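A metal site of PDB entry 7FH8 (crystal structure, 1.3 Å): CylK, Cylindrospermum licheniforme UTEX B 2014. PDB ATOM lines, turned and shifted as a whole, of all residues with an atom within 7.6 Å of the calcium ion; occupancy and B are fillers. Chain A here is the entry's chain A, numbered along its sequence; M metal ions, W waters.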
ATOM      1  N   THR A 458       6.630  13.903   7.789  1.00  0.00           N
ATOM      2  CA  THR A 458       7.775  14.636   8.281  1.00  0.00           C
ATOM      3  C   THR A 458       8.479  15.351   7.139  1.00  0.00           C
ATOM      4  O   THR A 458       8.545  14.825   6.019  1.00  0.00           O
ATOM      5  CB  THR A 458       8.782  13.737   9.038  1.00  0.00           C
ATOM      6  OG1 THR A 458       9.850  14.543   9.544  1.00  0.00           O
ATOM      7  CG2 THR A 458       9.362  12.637   8.143  1.00  0.00           C
ATOM      8  N   ASN A 466      15.770  11.442   4.294  1.00  0.00           N
ATOM      9  CA  ASN A 466      14.786  11.966   3.349  1.00  0.00           C
ATOM     10  C   ASN A 466      15.507  12.204   2.026  1.00  0.00           C
ATOM     11  O   ASN A 466      16.542  12.859   1.994  1.00  0.00           O
ATOM     12  CB  ASN A 466      14.255  13.277   3.921  1.00  0.00           C
ATOM     13  CG  ASN A 466      13.010  13.763   3.220  1.00  0.00           C
ATOM     14  OD1 ASN A 466      12.921  13.703   1.989  1.00  0.00           O
ATOM     15  ND2 ASN A 466      12.026  14.222   3.996  1.00  0.00           N
ATOM     16  N   THR A 467      14.967  11.659   0.920  1.00  0.00           N
ATOM     17  CA  THR A 467      15.594  11.821  -0.389  1.00  0.00           C
ATOM     18  C   THR A 467      15.155  13.095  -1.106  1.00  0.00           C
ATOM     19  O   THR A 467      15.693  13.386  -2.180  1.00  0.00           O
ATOM     20  CB  THR A 467      15.300  10.631  -1.308  1.00  0.00           C
ATOM     21  OG1 THR A 467      13.894  10.561  -1.583  1.00  0.00           O
ATOM     22  CG2 THR A 467      15.776   9.329  -0.674  1.00  0.00           C
ATOM     23  N   GLY A 468      14.180  13.816  -0.579  1.00  0.00           N
ATOM     24  CA  GLY A 468      13.886  15.126  -1.117  1.00  0.00           C
ATOM     25  C   GLY A 468      15.048  16.077  -0.915  1.00  0.00           C
ATOM     26  O   GLY A 468      15.794  15.985   0.057  1.00  0.00           O
ATOM     27  N   GLY A 471      13.241  19.334   1.743  1.00  0.00           N
ATOM     28  CA  GLY A 471      12.352  19.100   2.865  1.00  0.00           C
ATOM     29  C   GLY A 471      10.946  18.706   2.501  1.00  0.00           C
ATOM     30  O   GLY A 471      10.030  18.894   3.298  1.00  0.00           O
ATOM     31  N   GLU A 472      10.731  18.161   1.301  1.00  0.00           N
ATOM     32  CA  GLU A 472       9.419  17.623   0.951  1.00  0.00           C
ATOM     33  C   GLU A 472       9.022  16.515   1.924  1.00  0.00           C
ATOM     34  O   GLU A 472       9.866  15.809   2.474  1.00  0.00           O
ATOM     35  CB  GLU A 472       9.443  17.075  -0.476  1.00  0.00           C
ATOM     36  CG  GLU A 472       9.673  18.130  -1.578  1.00  0.00           C
ATOM     37  CD  GLU A 472      11.132  18.449  -1.868  1.00  0.00           C
ATOM     38  OE1 GLU A 472      12.050  17.993  -1.157  1.00  0.00           O
ATOM     39  OE2 GLU A 472      11.370  19.179  -2.862  1.00  0.00           O
ATOM     40  N   TYR A 473       7.709  16.359   2.127  1.00  0.00           N
ATOM     41  CA  TYR A 473       7.234  15.400   3.125  1.00  0.00           C
ATOM     42  C   TYR A 473       7.589  13.972   2.718  1.00  0.00           C
ATOM     43  O   TYR A 473       7.554  13.613   1.541  1.00  0.00           O
ATOM     44  CB  TYR A 473       5.709  15.445   3.260  1.00  0.00           C
ATOM     45  CG  TYR A 473       5.107  16.671   3.916  1.00  0.00           C
ATOM     46  CD1 TYR A 473       5.836  17.826   4.146  1.00  0.00           C
ATOM     47  CD2 TYR A 473       3.769  16.654   4.288  1.00  0.00           C
ATOM     48  CE1 TYR A 473       5.251  18.933   4.734  1.00  0.00           C
ATOM     49  CE2 TYR A 473       3.172  17.730   4.872  1.00  0.00           C
ATOM     50  CZ  TYR A 473       3.915  18.873   5.093  1.00  0.00           C
ATOM     51  OH  TYR A 473       3.348  19.977   5.669  1.00  0.00           O
ATOM     52  N   ASP A 474       7.890  13.166   3.731  1.00  0.00           N
ATOM     53  CA  ASP A 474       7.848  11.717   3.668  1.00  0.00           C
ATOM     54  C   ASP A 474       6.838  11.212   4.695  1.00  0.00           C
ATOM     55  O   ASP A 474       6.468  11.918   5.651  1.00  0.00           O
ATOM     56  CB  ASP A 474       9.196  11.084   4.041  1.00  0.00           C
ATOM     57  CG  ASP A 474      10.213  11.080   2.924  1.00  0.00           C
ATOM     58  OD1 ASP A 474       9.848  11.292   1.749  1.00  0.00           O
ATOM     59  OD2 ASP A 474      11.391  10.787   3.211  1.00  0.00           O
ATOM     60  N   ALA A 475       6.446   9.949   4.545  1.00  0.00           N
ATOM     61  CA  ALA A 475       5.609   9.269   5.523  1.00  0.00           C
ATOM     62  C   ALA A 475       6.488   8.575   6.563  1.00  0.00           C
ATOM     63  O   ALA A 475       7.582   8.099   6.252  1.00  0.00           O
ATOM     64  CB  ALA A 475       4.746   8.228   4.828  1.00  0.00           C
ATOM     65  N   GLN A 491      10.496   5.156   7.787  1.00  0.00           N
ATOM     66  CA  GLN A 491      10.160   6.300   6.945  1.00  0.00           C
ATOM     67  C   GLN A 491      10.230   5.840   5.499  1.00  0.00           C
ATOM     68  O   GLN A 491      11.120   5.060   5.136  1.00  0.00           O
ATOM     69  CB  GLN A 491      11.114   7.467   7.219  1.00  0.00           C
ATOM     70  CG  GLN A 491      10.868   8.706   6.376  1.00  0.00           C
ATOM     71  CD  GLN A 491      11.616   9.908   6.915  1.00  0.00           C
ATOM     72  OE1 GLN A 491      11.847  10.001   8.125  1.00  0.00           O
ATOM     73  NE2 GLN A 491      11.955  10.845   6.043  1.00  0.00           N
ATOM     74  N   PHE A 492       9.280   6.300   4.688  1.00  0.00           N
ATOM     75  CA  PHE A 492       9.253   5.920   3.281  1.00  0.00           C
ATOM     76  C   PHE A 492       8.708   7.084   2.467  1.00  0.00           C
ATOM     77  O   PHE A 492       8.001   7.953   2.983  1.00  0.00           O
ATOM     78  CB  PHE A 492       8.456   4.620   3.014  1.00  0.00           C
ATOM     79  CG  PHE A 492       7.012   4.654   3.490  1.00  0.00           C
ATOM     80  CD1 PHE A 492       6.701   4.379   4.809  1.00  0.00           C
ATOM     81  CD2 PHE A 492       5.975   4.918   2.609  1.00  0.00           C
ATOM     82  CE1 PHE A 492       5.364   4.376   5.252  1.00  0.00           C
ATOM     83  CE2 PHE A 492       4.645   4.946   3.047  1.00  0.00           C
ATOM     84  CZ  PHE A 492       4.347   4.665   4.370  1.00  0.00           C
ATOM     85  N   GLY A 493       9.074   7.119   1.201  1.00  0.00           N
ATOM     86  CA  GLY A 493       8.648   8.204   0.358  1.00  0.00           C
ATOM     87  C   GLY A 493       9.448   8.271  -0.918  1.00  0.00           C
ATOM     88  O   GLY A 493      10.336   7.446  -1.183  1.00  0.00           O
ATOM     89  N   THR A 494       9.091   9.257  -1.731  1.00  0.00           N
ATOM     90  CA  THR A 494       9.793   9.655  -2.949  1.00  0.00           C
ATOM     91  C   THR A 494      10.510  10.969  -2.667  1.00  0.00           C
ATOM     92  O   THR A 494      10.353  11.563  -1.596  1.00  0.00           O
ATOM     93  CB  THR A 494       8.781   9.868  -4.085  1.00  0.00           C
ATOM     94  OG1 THR A 494       8.005  11.043  -3.816  1.00  0.00           O
ATOM     95  CG2 THR A 494       7.870   8.669  -4.255  1.00  0.00           C
ATOM     96  N   PRO A 495      11.304  11.479  -3.613  1.00  0.00           N
ATOM     97  CA  PRO A 495      11.868  12.835  -3.446  1.00  0.00           C
ATOM     98  C   PRO A 495      10.829  13.943  -3.482  1.00  0.00           C
ATOM     99  O   PRO A 495      11.163  15.085  -3.137  1.00  0.00           O
ATOM    100  CB  PRO A 495      12.860  12.954  -4.622  1.00  0.00           C
ATOM    101  CG  PRO A 495      13.213  11.516  -4.932  1.00  0.00           C
ATOM    102  CD  PRO A 495      11.916  10.782  -4.763  1.00  0.00           C
ATOM    103  N   ASN A 496       9.594  13.655  -3.889  1.00  0.00           N
ATOM    104  CA  ASN A 496       8.528  14.641  -3.905  1.00  0.00           C
ATOM    105  C   ASN A 496       7.733  14.536  -2.595  1.00  0.00           C
ATOM    106  O   ASN A 496       8.094  13.787  -1.693  1.00  0.00           O
ATOM    107  CB  ASN A 496       7.656  14.434  -5.147  1.00  0.00           C
ATOM    108  CG  ASN A 496       6.993  15.727  -5.635  1.00  0.00           C
ATOM    109  OD1 ASN A 496       6.652  16.618  -4.844  1.00  0.00           O
ATOM    110  ND2 ASN A 496       6.806  15.823  -6.948  1.00  0.00           N
ATOM    111  N   TYR A 497       6.627  15.274  -2.496  1.00  0.00           N
ATOM    112  CA  TYR A 497       5.743  15.147  -1.343  1.00  0.00           C
ATOM    113  C   TYR A 497       4.998  13.818  -1.357  1.00  0.00           C
ATOM    114  O   TYR A 497       4.415  13.438  -2.378  1.00  0.00           O
ATOM    115  CB  TYR A 497       4.725  16.287  -1.298  1.00  0.00           C
ATOM    116  CG  TYR A 497       5.328  17.630  -0.917  1.00  0.00           C
ATOM    117  CD1 TYR A 497       5.857  18.472  -1.888  1.00  0.00           C
ATOM    118  CD2 TYR A 497       5.399  18.016   0.415  1.00  0.00           C
ATOM    119  CE1 TYR A 497       6.419  19.681  -1.538  1.00  0.00           C
ATOM    120  CE2 TYR A 497       5.954  19.231   0.769  1.00  0.00           C
ATOM    121  CZ  TYR A 497       6.462  20.056  -0.212  1.00  0.00           C
ATOM    122  OH  TYR A 497       7.025  21.265   0.138  1.00  0.00           O
ATOM    123  N   ASP A 498       5.021  13.133  -0.212  1.00  0.00           N
ATOM    124  CA  ASP A 498       4.169  11.989   0.068  1.00  0.00           C
ATOM    125  C   ASP A 498       3.503  12.293   1.405  1.00  0.00           C
ATOM    126  O   ASP A 498       4.144  12.815   2.314  1.00  0.00           O
ATOM    127  CB  ASP A 498       4.992  10.707   0.188  1.00  0.00           C
ATOM    128  CG  ASP A 498       6.158  10.686  -0.787  1.00  0.00           C
ATOM    129  OD1 ASP A 498       5.940  10.407  -1.989  1.00  0.00           O
ATOM    130  OD2 ASP A 498       7.302  10.988  -0.382  1.00  0.00           O
ATOM    131  N   PHE A 499       2.213  11.954   1.513  1.00  0.00           N
ATOM    132  CA  PHE A 499       1.392  12.448   2.613  1.00  0.00           C
ATOM    133  C   PHE A 499       0.520  11.296   3.097  1.00  0.00           C
ATOM    134  O   PHE A 499      -0.250  10.739   2.320  1.00  0.00           O
ATOM    135  CB  PHE A 499       0.520  13.592   2.097  1.00  0.00           C
ATOM    136  CG  PHE A 499      -0.205  14.393   3.164  1.00  0.00           C
ATOM    137  CD1 PHE A 499      -1.300  13.863   3.841  1.00  0.00           C
ATOM    138  CD2 PHE A 499       0.186  15.703   3.432  1.00  0.00           C
ATOM    139  CE1 PHE A 499      -1.971  14.610   4.814  1.00  0.00           C
ATOM    140  CE2 PHE A 499      -0.473  16.452   4.398  1.00  0.00           C
ATOM    141  CZ  PHE A 499      -1.560  15.908   5.082  1.00  0.00           C
ATOM    142  N   THR A 517       0.655  10.520  -3.080  1.00  0.00           N
ATOM    143  CA  THR A 517       2.015  10.867  -3.472  1.00  0.00           C
ATOM    144  C   THR A 517       1.970  11.649  -4.772  1.00  0.00           C
ATOM    145  O   THR A 517       1.122  11.410  -5.623  1.00  0.00           O
ATOM    146  CB  THR A 517       2.898   9.614  -3.631  1.00  0.00           C
ATOM    147  OG1 THR A 517       4.229  10.017  -3.982  1.00  0.00           O
ATOM    148  CG2 THR A 517       2.362   8.686  -4.720  1.00  0.00           C
ATOM    149  N   LEU A 521       5.930   6.182  -5.878  1.00  0.00           N
ATOM    150  CA  LEU A 521       6.164   5.528  -4.597  1.00  0.00           C
ATOM    151  C   LEU A 521       6.000   4.011  -4.699  1.00  0.00           C
ATOM    152  O   LEU A 521       6.907   3.255  -4.345  1.00  0.00           O
ATOM    153  CB  LEU A 521       5.251   6.123  -3.523  1.00  0.00           C
ATOM    154  CG  LEU A 521       5.481   5.599  -2.098  1.00  0.00           C
ATOM    155  CD1 LEU A 521       6.931   5.812  -1.640  1.00  0.00           C
ATOM    156  CD2 LEU A 521       4.504   6.250  -1.126  1.00  0.00           C
HETATM  157 CA    CA M   1       8.971  12.504   0.016  1.00  0.00          CA
HETATM  158  O   HOH W   1      10.756  13.988   0.435  1.00  0.00           O
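Water W1 bridges OD1 of Asn 466 (2.7 Å) and O of Glu 472 (2.9 Å).
The backbone NH (N) of Asp 474 sits at hydrogen-bond distance from the backbone carbonyl oxygen (O) of Thr 458 (2.9 Å).
OD2 of Asp 474 sits at hydrogen-bond distance from NE2 of Gln 491, 2.9 Å away.
OD1 of Asp 498 is in hydrogen-bond range of OG1 of Thr 517 (2.7 Å).
N of Asn 496 sits at hydrogen-bond distance from OG1 of Thr 494.
OD1 of Asp 474 binds the calcium ion, at 2.3 Å.
The calcium ion is bound by OD2 of Asp 498.
The calcium ion is bound by O of Asn 496.
The calcium ion is bound by the backbone carbonyl oxygen (O) of Thr 494 (2.3 Å).
Water W1 binds the calcium ion, 2.4 Å away.
The calcium ion is bound by O of Tyr 473 (2.4 Å).
The calcium ion has six donor atoms within binding distance.
The nearest printed residue that does not touch the calcium ion is Pro 495 (4.2 Å).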
